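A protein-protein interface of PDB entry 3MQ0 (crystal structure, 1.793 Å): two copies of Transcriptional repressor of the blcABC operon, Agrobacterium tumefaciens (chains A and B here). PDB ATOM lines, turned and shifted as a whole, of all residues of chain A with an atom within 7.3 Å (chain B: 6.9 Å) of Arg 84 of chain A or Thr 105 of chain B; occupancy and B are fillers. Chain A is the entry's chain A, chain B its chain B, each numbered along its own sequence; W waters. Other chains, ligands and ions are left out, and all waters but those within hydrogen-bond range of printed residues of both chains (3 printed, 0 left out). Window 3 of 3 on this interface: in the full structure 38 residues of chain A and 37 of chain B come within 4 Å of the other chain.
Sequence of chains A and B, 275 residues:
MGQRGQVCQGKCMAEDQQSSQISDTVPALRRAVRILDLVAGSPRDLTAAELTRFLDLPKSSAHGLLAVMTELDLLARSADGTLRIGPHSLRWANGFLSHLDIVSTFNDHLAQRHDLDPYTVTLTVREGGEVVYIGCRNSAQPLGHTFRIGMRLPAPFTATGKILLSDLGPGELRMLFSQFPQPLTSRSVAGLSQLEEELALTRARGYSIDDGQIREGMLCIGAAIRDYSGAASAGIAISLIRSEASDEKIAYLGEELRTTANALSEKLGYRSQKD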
ATOM      1  N   LEU A  36     -16.684  19.751  21.547  1.00  0.00           N
ATOM      2  CA  LEU A  36     -17.638  19.014  20.742  1.00  0.00           C
ATOM      3  C   LEU A  36     -18.816  19.888  20.322  1.00  0.00           C
ATOM      4  O   LEU A  36     -19.281  19.806  19.176  1.00  0.00           O
ATOM      5  CB  LEU A  36     -18.119  17.764  21.475  1.00  0.00           C
ATOM      6  CG  LEU A  36     -17.041  16.707  21.645  1.00  0.00           C
ATOM      7  CD1 LEU A  36     -17.564  15.605  22.599  1.00  0.00           C
ATOM      8  CD2 LEU A  36     -16.645  16.125  20.282  1.00  0.00           C
ATOM      9  N   VAL A  39     -17.481  22.308  17.522  1.00  0.00           N
ATOM     10  CA  VAL A  39     -17.206  21.574  16.293  1.00  0.00           C
ATOM     11  C   VAL A  39     -18.503  21.136  15.619  1.00  0.00           C
ATOM     12  O   VAL A  39     -18.652  21.257  14.398  1.00  0.00           O
ATOM     13  CB  VAL A  39     -16.276  20.376  16.541  1.00  0.00           C
ATOM     14  CG1 VAL A  39     -16.219  19.457  15.312  1.00  0.00           C
ATOM     15  CG2 VAL A  39     -14.871  20.865  16.916  1.00  0.00           C
ATOM     16  N   ALA A  40     -19.453  20.672  16.423  1.00  0.00           N
ATOM     17  CA  ALA A  40     -20.727  20.188  15.901  1.00  0.00           C
ATOM     18  C   ALA A  40     -21.549  21.320  15.290  1.00  0.00           C
ATOM     19  O   ALA A  40     -22.255  21.111  14.306  1.00  0.00           O
ATOM     20  CB  ALA A  40     -21.529  19.473  17.003  1.00  0.00           C
ATOM     21  N   ASP A  45     -15.114  23.475   8.986  1.00  0.00           N
ATOM     22  CA  ASP A  45     -14.183  22.713   9.820  1.00  0.00           C
ATOM     23  C   ASP A  45     -13.100  23.625  10.399  1.00  0.00           C
ATOM     24  O   ASP A  45     -12.572  24.494   9.709  1.00  0.00           O
ATOM     25  CB  ASP A  45     -13.547  21.558   9.037  1.00  0.00           C
ATOM     26  CG  ASP A  45     -14.552  20.475   8.666  1.00  0.00           C
ATOM     27  OD1 ASP A  45     -15.559  20.318   9.392  1.00  0.00           O
ATOM     28  OD2 ASP A  45     -14.332  19.779   7.649  1.00  0.00           O
ATOM     29  N   LEU A  46     -12.770  23.420  11.669  1.00  0.00           N
ATOM     30  CA  LEU A  46     -11.835  24.289  12.370  1.00  0.00           C
ATOM     31  C   LEU A  46     -10.527  23.574  12.671  1.00  0.00           C
ATOM     32  O   LEU A  46     -10.521  22.365  12.907  1.00  0.00           O
ATOM     33  CB  LEU A  46     -12.456  24.761  13.682  1.00  0.00           C
ATOM     34  CG  LEU A  46     -13.686  25.652  13.551  1.00  0.00           C
ATOM     35  CD1 LEU A  46     -14.212  26.004  14.934  1.00  0.00           C
ATOM     36  CD2 LEU A  46     -13.341  26.914  12.772  1.00  0.00           C
ATOM     37  N   LEU A  51      -9.822  26.428  17.216  1.00  0.00           N
ATOM     38  CA  LEU A  51     -10.624  25.942  18.341  1.00  0.00           C
ATOM     39  C   LEU A  51     -10.124  26.510  19.654  1.00  0.00           C
ATOM     40  O   LEU A  51     -10.907  26.971  20.483  1.00  0.00           O
ATOM     41  CB  LEU A  51     -10.586  24.413  18.423  1.00  0.00           C
ATOM     42  CG  LEU A  51     -11.606  23.630  17.608  1.00  0.00           C
ATOM     43  CD1 LEU A  51     -11.269  22.144  17.632  1.00  0.00           C
ATOM     44  CD2 LEU A  51     -12.994  23.876  18.176  1.00  0.00           C
ATOM     45  N   THR A  70      -9.054  12.881  19.741  1.00  0.00           N
ATOM     46  CA  THR A  70      -8.861  12.304  18.416  1.00  0.00           C
ATOM     47  C   THR A  70      -8.574  10.805  18.524  1.00  0.00           C
ATOM     48  O   THR A  70      -9.119  10.003  17.772  1.00  0.00           O
ATOM     49  CB  THR A  70      -7.719  13.014  17.661  1.00  0.00           C
ATOM     50  OG1 THR A  70      -8.034  14.408  17.530  1.00  0.00           O
ATOM     51  CG2 THR A  70      -7.525  12.421  16.279  1.00  0.00           C
ATOM     52  N   ASP A  73     -11.553   8.849  18.923  1.00  0.00           N
ATOM     53  CA  ASP A  73     -12.498   9.033  17.824  1.00  0.00           C
ATOM     54  C   ASP A  73     -13.695   9.908  18.177  1.00  0.00           C
ATOM     55  O   ASP A  73     -14.736   9.830  17.524  1.00  0.00           O
ATOM     56  CB  ASP A  73     -12.982   7.688  17.280  1.00  0.00           C
ATOM     57  CG  ASP A  73     -11.895   6.938  16.535  1.00  0.00           C
ATOM     58  OD1 ASP A  73     -11.196   7.566  15.702  1.00  0.00           O
ATOM     59  OD2 ASP A  73     -11.735   5.726  16.796  1.00  0.00           O
ATOM     60  N   LEU A  74     -13.535  10.755  19.184  1.00  0.00           N
ATOM     61  CA  LEU A  74     -14.511  11.805  19.468  1.00  0.00           C
ATOM     62  C   LEU A  74     -14.420  12.889  18.399  1.00  0.00           C
ATOM     63  O   LEU A  74     -15.427  13.491  18.015  1.00  0.00           O
ATOM     64  CB  LEU A  74     -14.258  12.416  20.851  1.00  0.00           C
ATOM     65  CG  LEU A  74     -14.452  11.498  22.065  1.00  0.00           C
ATOM     66  CD1 LEU A  74     -14.325  12.271  23.387  1.00  0.00           C
ATOM     67  CD2 LEU A  74     -15.795  10.828  21.967  1.00  0.00           C
ATOM     68  N   LEU A  75     -13.197  13.154  17.951  1.00  0.00           N
ATOM     69  CA  LEU A  75     -12.950  14.059  16.827  1.00  0.00           C
ATOM     70  C   LEU A  75     -12.262  13.277  15.739  1.00  0.00           C
ATOM     71  O   LEU A  75     -11.680  12.238  16.014  1.00  0.00           O
ATOM     72  CB  LEU A  75     -12.021  15.195  17.252  1.00  0.00           C
ATOM     73  CG  LEU A  75     -12.603  16.092  18.332  1.00  0.00           C
ATOM     74  CD1 LEU A  75     -11.558  17.061  18.841  1.00  0.00           C
ATOM     75  CD2 LEU A  75     -13.836  16.825  17.814  1.00  0.00           C
ATOM     76  N   ALA A  76     -12.326  13.781  14.509  1.00  0.00           N
ATOM     77  CA  ALA A  76     -11.535  13.228  13.426  1.00  0.00           C
ATOM     78  C   ALA A  76     -10.724  14.358  12.804  1.00  0.00           C
ATOM     79  O   ALA A  76     -11.243  15.448  12.587  1.00  0.00           O
ATOM     80  CB  ALA A  76     -12.419  12.573  12.387  1.00  0.00           C
ATOM     81  N   ARG A  77      -9.449  14.091  12.557  1.00  0.00           N
ATOM     82  CA  ARG A  77      -8.564  15.079  11.991  1.00  0.00           C
ATOM     83  C   ARG A  77      -8.370  14.812  10.506  1.00  0.00           C
ATOM     84  O   ARG A  77      -7.970  13.717  10.107  1.00  0.00           O
ATOM     85  CB  ARG A  77      -7.211  15.053  12.697  1.00  0.00           C
ATOM     86  CG  ARG A  77      -6.276  16.166  12.282  1.00  0.00           C
ATOM     87  CD  ARG A  77      -4.926  15.982  12.953  1.00  0.00           C
ATOM     88  NE  ARG A  77      -4.020  17.088  12.673  1.00  0.00           N
ATOM     89  CZ  ARG A  77      -3.265  17.174  11.581  1.00  0.00           C
ATOM     90  NH1 ARG A  77      -3.319  16.219  10.660  1.00  0.00           N
ATOM     91  NH2 ARG A  77      -2.465  18.219  11.408  1.00  0.00           N
ATOM     92  N   SER A  78      -8.657  15.825   9.704  1.00  0.00           N
ATOM     93  CA  SER A  78      -8.488  15.761   8.258  1.00  0.00           C
ATOM     94  C   SER A  78      -7.034  16.041   7.875  1.00  0.00           C
ATOM     95  O   SER A  78      -6.266  16.603   8.665  1.00  0.00           O
ATOM     96  CB  SER A  78      -9.415  16.775   7.589  1.00  0.00           C
ATOM     97  OG  SER A  78      -9.195  16.844   6.190  1.00  0.00           O
ATOM     98  N   GLY A  81      -5.607  19.320   8.542  1.00  0.00           N
ATOM     99  CA  GLY A  81      -5.468  19.716   9.934  1.00  0.00           C
ATOM    100  C   GLY A  81      -6.760  20.136  10.608  1.00  0.00           C
ATOM    101  O   GLY A  81      -6.764  20.474  11.793  1.00  0.00           O
ATOM    102  N   THR A  82      -7.862  20.110   9.867  1.00  0.00           N
ATOM    103  CA  THR A  82      -9.131  20.545  10.422  1.00  0.00           C
ATOM    104  C   THR A  82      -9.785  19.397  11.152  1.00  0.00           C
ATOM    105  O   THR A  82      -9.575  18.232  10.816  1.00  0.00           O
ATOM    106  CB  THR A  82     -10.088  21.092   9.353  1.00  0.00           C
ATOM    107  OG1 THR A  82     -10.294  20.106   8.336  1.00  0.00           O
ATOM    108  CG2 THR A  82      -9.513  22.352   8.722  1.00  0.00           C
ATOM    109  N   LEU A  83     -10.577  19.744  12.156  1.00  0.00           N
ATOM    110  CA  LEU A  83     -11.216  18.762  13.009  1.00  0.00           C
ATOM    111  C   LEU A  83     -12.713  18.703  12.767  1.00  0.00           C
ATOM    112  O   LEU A  83     -13.370  19.716  12.538  1.00  0.00           O
ATOM    113  CB  LEU A  83     -10.927  19.100  14.468  1.00  0.00           C
ATOM    114  CG  LEU A  83      -9.433  18.968  14.774  1.00  0.00           C
ATOM    115  CD1 LEU A  83      -9.052  19.773  15.986  1.00  0.00           C
ATOM    116  CD2 LEU A  83      -9.054  17.512  14.960  1.00  0.00           C
ATOM    117  N   ARG A  84     -13.254  17.500  12.820  1.00  0.00           N
ATOM    118  CA  ARG A  84     -14.681  17.327  12.653  1.00  0.00           C
ATOM    119  C   ARG A  84     -15.119  16.377  13.748  1.00  0.00           C
ATOM    120  O   ARG A  84     -14.281  15.798  14.437  1.00  0.00           O
ATOM    121  CB  ARG A  84     -14.978  16.740  11.274  1.00  0.00           C
ATOM    122  CG  ARG A  84     -14.208  15.471  10.973  1.00  0.00           C
ATOM    123  CD  ARG A  84     -14.335  15.044   9.503  1.00  0.00           C
ATOM    124  NE  ARG A  84     -13.916  13.653   9.337  1.00  0.00           N
ATOM    125  CZ  ARG A  84     -13.950  12.977   8.193  1.00  0.00           C
ATOM    126  NH1 ARG A  84     -14.381  13.565   7.080  1.00  0.00           N
ATOM    127  NH2 ARG A  84     -13.547  11.710   8.166  1.00  0.00           N
ATOM    128  N   ILE A  85     -16.422  16.222  13.925  1.00  0.00           N
ATOM    129  CA  ILE A  85     -16.905  15.245  14.885  1.00  0.00           C
ATOM    130  C   ILE A  85     -16.551  13.865  14.367  1.00  0.00           C
ATOM    131  O   ILE A  85     -16.717  13.582  13.169  1.00  0.00           O
ATOM    132  CB  ILE A  85     -18.415  15.346  15.084  1.00  0.00           C
ATOM    133  CG1 ILE A  85     -18.802  16.744  15.582  1.00  0.00           C
ATOM    134  CG2 ILE A  85     -18.890  14.279  16.053  1.00  0.00           C
ATOM    135  CD1 ILE A  85     -18.280  17.100  16.974  1.00  0.00           C
ATOM    136  N   GLY A  86     -16.043  13.011  15.252  1.00  0.00           N
ATOM    137  CA  GLY A  86     -15.706  11.645  14.890  1.00  0.00           C
ATOM    138  C   GLY A  86     -16.900  10.720  15.091  1.00  0.00           C
ATOM    139  O   GLY A  86     -17.934  11.144  15.595  1.00  0.00           O
ATOM    140  N   PRO A  87     -16.750   9.446  14.723  1.00  0.00           N
ATOM    141  CA  PRO A  87     -17.869   8.493  14.758  1.00  0.00           C
ATOM    142  C   PRO A  87     -18.301   8.057  16.158  1.00  0.00           C
ATOM    143  O   PRO A  87     -19.429   7.583  16.309  1.00  0.00           O
ATOM    144  CB  PRO A  87     -17.329   7.284  13.969  1.00  0.00           C
ATOM    145  CG  PRO A  87     -15.851   7.380  14.086  1.00  0.00           C
ATOM    146  CD  PRO A  87     -15.520   8.852  14.164  1.00  0.00           C
ATOM    147  N   GLY B  95     -24.176  16.407  14.239  1.00  0.00           N
ATOM    148  CA  GLY B  95     -23.048  17.121  13.677  1.00  0.00           C
ATOM    149  C   GLY B  95     -22.167  16.200  12.848  1.00  0.00           C
ATOM    150  O   GLY B  95     -21.710  16.578  11.773  1.00  0.00           O
ATOM    151  N   PHE B  96     -21.930  14.992  13.350  1.00  0.00           N
ATOM    152  CA  PHE B  96     -21.200  13.995  12.587  1.00  0.00           C
ATOM    153  C   PHE B  96     -21.881  13.707  11.248  1.00  0.00           C
ATOM    154  O   PHE B  96     -21.240  13.771  10.198  1.00  0.00           O
ATOM    155  CB  PHE B  96     -21.036  12.700  13.392  1.00  0.00           C
ATOM    156  CG  PHE B  96     -20.435  11.560  12.602  1.00  0.00           C
ATOM    157  CD1 PHE B  96     -19.069  11.513  12.342  1.00  0.00           C
ATOM    158  CD2 PHE B  96     -21.232  10.529  12.136  1.00  0.00           C
ATOM    159  CE1 PHE B  96     -18.517  10.470  11.631  1.00  0.00           C
ATOM    160  CE2 PHE B  96     -20.691   9.478  11.416  1.00  0.00           C
ATOM    161  CZ  PHE B  96     -19.329   9.444  11.158  1.00  0.00           C
ATOM    162  N   HIS B  99     -21.765  16.761   8.669  1.00  0.00           N
ATOM    163  CA  HIS B  99     -20.461  17.118   8.131  1.00  0.00           C
ATOM    164  C   HIS B  99     -19.824  15.979   7.328  1.00  0.00           C
ATOM    165  O   HIS B  99     -18.707  16.119   6.836  1.00  0.00           O
ATOM    166  CB  HIS B  99     -19.516  17.534   9.261  1.00  0.00           C
ATOM    167  CG  HIS B  99     -19.831  18.873   9.860  1.00  0.00           C
ATOM    168  ND1 HIS B  99     -21.083  19.200  10.334  1.00  0.00           N
ATOM    169  CD2 HIS B  99     -19.051  19.960  10.072  1.00  0.00           C
ATOM    170  CE1 HIS B  99     -21.063  20.435  10.806  1.00  0.00           C
ATOM    171  NE2 HIS B  99     -19.841  20.917  10.659  1.00  0.00           N
ATOM    172  N   LEU B 100     -20.532  14.861   7.202  1.00  0.00           N
ATOM    173  CA  LEU B 100     -19.975  13.673   6.550  1.00  0.00           C
ATOM    174  C   LEU B 100     -19.697  13.894   5.062  1.00  0.00           C
ATOM    175  O   LEU B 100     -20.598  14.215   4.288  1.00  0.00           O
ATOM    176  CB  LEU B 100     -20.900  12.467   6.746  1.00  0.00           C
ATOM    177  CG  LEU B 100     -20.259  11.075   6.702  1.00  0.00           C
ATOM    178  CD1 LEU B 100     -19.090  10.996   7.669  1.00  0.00           C
ATOM    179  CD2 LEU B 100     -21.291  10.000   7.012  1.00  0.00           C
ATOM    180  N   ASP B 101     -18.436  13.714   4.674  1.00  0.00           N
ATOM    181  CA  ASP B 101     -17.998  13.900   3.294  1.00  0.00           C
ATOM    182  C   ASP B 101     -17.155  12.690   2.918  1.00  0.00           C
ATOM    183  O   ASP B 101     -15.976  12.622   3.247  1.00  0.00           O
ATOM    184  CB  ASP B 101     -17.164  15.172   3.179  1.00  0.00           C
ATOM    185  CG  ASP B 101     -16.805  15.522   1.736  1.00  0.00           C
ATOM    186  OD1 ASP B 101     -16.670  14.607   0.893  1.00  0.00           O
ATOM    187  OD2 ASP B 101     -16.652  16.728   1.447  1.00  0.00           O
ATOM    188  N   ILE B 102     -17.772  11.733   2.245  1.00  0.00           N
ATOM    189  CA  ILE B 102     -17.110  10.467   1.962  1.00  0.00           C
ATOM    190  C   ILE B 102     -15.866  10.630   1.068  1.00  0.00           C
ATOM    191  O   ILE B 102     -14.860   9.944   1.253  1.00  0.00           O
ATOM    192  CB  ILE B 102     -18.102   9.448   1.371  1.00  0.00           C
ATOM    193  CG1 ILE B 102     -17.454   8.080   1.233  1.00  0.00           C
ATOM    194  CG2 ILE B 102     -18.657   9.932   0.038  1.00  0.00           C
ATOM    195  CD1 ILE B 102     -18.381   7.056   0.642  1.00  0.00           C
ATOM    196  N   VAL B 103     -15.919  11.552   0.115  1.00  0.00           N
ATOM    197  CA  VAL B 103     -14.796  11.711  -0.788  1.00  0.00           C
ATOM    198  C   VAL B 103     -13.555  12.212  -0.053  1.00  0.00           C
ATOM    199  O   VAL B 103     -12.456  11.714  -0.281  1.00  0.00           O
ATOM    200  CB  VAL B 103     -15.145  12.657  -1.951  1.00  0.00           C
ATOM    201  CG1 VAL B 103     -13.909  12.946  -2.801  1.00  0.00           C
ATOM    202  CG2 VAL B 103     -16.265  12.049  -2.787  1.00  0.00           C
ATOM    203  N   SER B 104     -13.705  13.204   0.821  1.00  0.00           N
ATOM    204  CA  SER B 104     -12.535  13.693   1.551  1.00  0.00           C
ATOM    205  C   SER B 104     -12.037  12.638   2.561  1.00  0.00           C
ATOM    206  O   SER B 104     -10.841  12.499   2.772  1.00  0.00           O
ATOM    207  CB  SER B 104     -12.812  15.034   2.242  1.00  0.00           C
ATOM    208  OG  SER B 104     -13.858  14.918   3.188  1.00  0.00           O
ATOM    209  N   THR B 105     -12.959  11.894   3.166  1.00  0.00           N
ATOM    210  CA  THR B 105     -12.595  10.801   4.068  1.00  0.00           C
ATOM    211  C   THR B 105     -11.771   9.740   3.325  1.00  0.00           C
ATOM    212  O   THR B 105     -10.732   9.286   3.798  1.00  0.00           O
ATOM    213  CB  THR B 105     -13.863  10.151   4.670  1.00  0.00           C
ATOM    214  OG1 THR B 105     -14.577  11.137   5.431  1.00  0.00           O
ATOM    215  CG2 THR B 105     -13.506   8.970   5.569  1.00  0.00           C
ATOM    216  N   PHE B 106     -12.257   9.365   2.151  1.00  0.00           N
ATOM    217  CA  PHE B 106     -11.559   8.453   1.236  1.00  0.00           C
ATOM    218  C   PHE B 106     -10.147   8.967   0.912  1.00  0.00           C
ATOM    219  O   PHE B 106      -9.175   8.247   1.089  1.00  0.00           O
ATOM    220  CB  PHE B 106     -12.431   8.311  -0.016  1.00  0.00           C
ATOM    221  CG  PHE B 106     -11.732   7.746  -1.235  1.00  0.00           C
ATOM    222  CD1 PHE B 106     -11.552   6.375  -1.383  1.00  0.00           C
ATOM    223  CD2 PHE B 106     -11.346   8.581  -2.269  1.00  0.00           C
ATOM    224  CE1 PHE B 106     -10.951   5.850  -2.537  1.00  0.00           C
ATOM    225  CE2 PHE B 106     -10.739   8.072  -3.417  1.00  0.00           C
ATOM    226  CZ  PHE B 106     -10.546   6.700  -3.546  1.00  0.00           C
ATOM    227  N   ASN B 107     -10.032  10.218   0.466  1.00  0.00           N
ATOM    228  CA  ASN B 107      -8.732  10.765   0.068  1.00  0.00           C
ATOM    229  C   ASN B 107      -7.721  10.659   1.196  1.00  0.00           C
ATOM    230  O   ASN B 107      -6.587  10.219   0.991  1.00  0.00           O
ATOM    231  CB  ASN B 107      -8.841  12.237  -0.349  1.00  0.00           C
ATOM    232  CG  ASN B 107      -9.564  12.433  -1.667  1.00  0.00           C
ATOM    233  OD1 ASN B 107      -9.590  11.553  -2.507  1.00  0.00           O
ATOM    234  ND2 ASN B 107     -10.136  13.620  -1.856  1.00  0.00           N
ATOM    235  N   ASP B 108      -8.138  11.077   2.388  1.00  0.00           N
ATOM    236  CA  ASP B 108      -7.270  11.070   3.562  1.00  0.00           C
ATOM    237  C   ASP B 108      -6.871   9.663   4.010  1.00  0.00           C
ATOM    238  O   ASP B 108      -5.746   9.423   4.464  1.00  0.00           O
ATOM    239  CB  ASP B 108      -7.936  11.836   4.703  1.00  0.00           C
ATOM    240  CG  ASP B 108      -8.043  13.331   4.410  1.00  0.00           C
ATOM    241  OD1 ASP B 108      -7.413  13.794   3.430  1.00  0.00           O
ATOM    242  OD2 ASP B 108      -8.747  14.043   5.155  1.00  0.00           O
ATOM    243  N   HIS B 109      -7.798   8.734   3.871  1.00  0.00           N
ATOM    244  CA  HIS B 109      -7.524   7.346   4.184  1.00  0.00           C
ATOM    245  C   HIS B 109      -6.416   6.813   3.281  1.00  0.00           C
ATOM    246  O   HIS B 109      -5.529   6.093   3.735  1.00  0.00           O
ATOM    247  CB  HIS B 109      -8.799   6.526   4.002  1.00  0.00           C
ATOM    248  CG  HIS B 109      -8.746   5.168   4.622  1.00  0.00           C
ATOM    249  ND1 HIS B 109      -8.673   4.970   5.982  1.00  0.00           N
ATOM    250  CD2 HIS B 109      -8.791   3.929   4.065  1.00  0.00           C
ATOM    251  CE1 HIS B 109      -8.656   3.674   6.239  1.00  0.00           C
ATOM    252  NE2 HIS B 109      -8.733   3.023   5.091  1.00  0.00           N
ATOM    253  N   LEU B 110      -6.461   7.169   1.999  1.00  0.00           N
ATOM    254  CA  LEU B 110      -5.434   6.707   1.068  1.00  0.00           C
ATOM    255  C   LEU B 110      -4.065   7.314   1.373  1.00  0.00           C
ATOM    256  O   LEU B 110      -3.029   6.680   1.155  1.00  0.00           O
ATOM    257  CB  LEU B 110      -5.825   7.012  -0.373  1.00  0.00           C
ATOM    258  CG  LEU B 110      -6.993   6.195  -0.911  1.00  0.00           C
ATOM    259  CD1 LEU B 110      -7.197   6.514  -2.382  1.00  0.00           C
ATOM    260  CD2 LEU B 110      -6.712   4.726  -0.708  1.00  0.00           C
ATOM    261  N   ALA B 263     -12.197  -0.394   7.354  1.00  0.00           N
ATOM    262  CA  ALA B 263     -11.652   0.713   8.147  1.00  0.00           C
ATOM    263  C   ALA B 263     -12.255   2.037   7.693  1.00  0.00           C
ATOM    264  O   ALA B 263     -12.554   2.914   8.504  1.00  0.00           O
ATOM    265  CB  ALA B 263     -10.134   0.761   8.039  1.00  0.00           C
ATOM    266  N   LEU B 264     -12.448   2.188   6.390  1.00  0.00           N
ATOM    267  CA  LEU B 264     -13.091   3.394   5.884  1.00  0.00           C
ATOM    268  C   LEU B 264     -14.548   3.494   6.358  1.00  0.00           C
ATOM    269  O   LEU B 264     -15.005   4.572   6.747  1.00  0.00           O
ATOM    270  CB  LEU B 264     -13.025   3.421   4.349  1.00  0.00           C
ATOM    271  CG  LEU B 264     -13.354   4.713   3.610  1.00  0.00           C
ATOM    272  CD1 LEU B 264     -12.576   5.881   4.184  1.00  0.00           C
ATOM    273  CD2 LEU B 264     -13.037   4.552   2.127  1.00  0.00           C
ATOM    274  N   SER B 265     -15.269   2.375   6.311  1.00  0.00           N
ATOM    275  CA  SER B 265     -16.659   2.313   6.791  1.00  0.00           C
ATOM    276  C   SER B 265     -16.786   2.746   8.254  1.00  0.00           C
ATOM    277  O   SER B 265     -17.710   3.475   8.631  1.00  0.00           O
ATOM    278  CB  SER B 265     -17.202   0.883   6.639  1.00  0.00           C
ATOM    279  OG  SER B 265     -17.206   0.518   5.265  1.00  0.00           O
ATOM    280  N   LYS B 267     -14.934   4.830   9.782  1.00  0.00           N
ATOM    281  CA  LYS B 267     -14.817   6.279   9.821  1.00  0.00           C
ATOM    282  C   LYS B 267     -16.134   6.957   9.480  1.00  0.00           C
ATOM    283  O   LYS B 267     -16.334   8.106   9.828  1.00  0.00           O
ATOM    284  CB  LYS B 267     -13.712   6.746   8.869  1.00  0.00           C
ATOM    285  CG  LYS B 267     -12.329   6.332   9.321  1.00  0.00           C
ATOM    286  CD  LYS B 267     -11.259   6.850   8.371  1.00  0.00           C
ATOM    287  CE  LYS B 267      -9.863   6.560   8.919  1.00  0.00           C
ATOM    288  NZ  LYS B 267      -8.805   6.848   7.905  1.00  0.00           N
ATOM    289  N   LEU B 268     -17.031   6.235   8.811  1.00  0.00           N
ATOM    290  CA  LEU B 268     -18.308   6.797   8.384  1.00  0.00           C
ATOM    291  C   LEU B 268     -19.453   6.424   9.311  1.00  0.00           C
ATOM    292  O   LEU B 268     -20.613   6.764   9.050  1.00  0.00           O
ATOM    293  CB  LEU B 268     -18.629   6.369   6.948  1.00  0.00           C
ATOM    294  CG  LEU B 268     -17.589   6.732   5.891  1.00  0.00           C
ATOM    295  CD1 LEU B 268     -18.004   6.166   4.532  1.00  0.00           C
ATOM    296  CD2 LEU B 268     -17.413   8.241   5.814  1.00  0.00           C
HETATM  297  O   HOH W   1     -14.783  10.060  10.546  1.00  0.00           O
HETATM  298  O   HOH W   2     -16.798  12.321   6.359  1.00  0.00           O
HETATM  299  O   HOH W   3     -18.402  14.281  10.216  1.00  0.00           O
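The side-chain carboxylate (OD2) of Asp 108 of chain B lies within hydrogen-bond range of the side-chain hydroxyl (OG) of Ser 78 of chain A, at 3.0 Å.
The side-chain hydroxyl of Thr 105 of chain B is in hydrogen-bond range of the guanidinium group of Arg 84 of chain A.
The backbone carbonyl oxygen (O) of Leu 74 of chain A is in hydrogen-bond range of the backbone NH (N) of Gly 86 of chain A (2.9 Å).
N of Ala 76 of chain A lies within hydrogen-bond range of O of Arg 84 of chain A (2.8 Å).
ND1 of His 99 of chain B is in hydrogen-bond range of O of Gly 95 of chain B (3.1 Å).
O of Asp 101 of chain B lies within hydrogen-bond range of OG1 of Thr 105 of chain B (3.0 Å).
O of Val 39 of chain A touches NE2 of His 99 of chain B, 3.9 Å away.
His 99 of chain B touches Ala 40 of chain A (CE1 to O, 3.8 Å).
His 99 of chain B touches Asp 45 of chain A.
CD1 of Phe 96 of chain B touches O of Ile 85 of chain A, at 3.2 Å.
Phe 96 of chain B touches Gly 86 of chain A.
N of Pro 87 of chain A touches CE1 of Phe 96 of chain B, 3.7 Å away.
Leu 74 of chain A touches none of the printed residues of chain B.
Arg 84 of chain A touches just one residue of chain B: Thr 105 (2.9 Å).
Printed residues of chain B within 4 Å of Gly 86 of chain A: Phe 96 (3.5 Å).
Of the printed residues of chain B, Pro 87 of chain A touches Phe 96.
Of the printed residues of chain A, Phe 96 of chain B touches Ile 85 (3.2 Å), Gly 86 (3.5 Å) and Pro 87 (3.7 Å).
Thr 105 of chain B touches just one residue of chain A: Arg 84.
Printed residues of chain A within 4 Å of Asp 108 of chain B: Ser 78 (3.0 Å).
Along chain A the printed residues that touch a printed residue of chain B span positions 39 to 87.
Of the 19 printed residues of chain B, 4 touch a printed residue of chain A.
Hydrophobic or aromatic side chains of chain B within 4 Å of the printed part of chain A: Phe 96 and His 99.
No position is printed for both chains.
Of the 8 pairs that touch across the chains among the printed residues, none has its exchanged pair printed and touching as well.
Water W1 lies within hydrogen-bond range of the backbone carbonyl oxygen (O) of Lys 267 of chain B and the guanidinium group (NH2) of Arg 84 of chain A.
Water W2 lies within hydrogen-bond range of OG1 of Thr 105 of chain B, N of Asp 101 of chain B and NH1 of Arg 84 of chain A.
Water W3 bridges O of Phe 96 of chain B (2.9 Å) and O of Ile 85 of chain A (3.5 Å).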
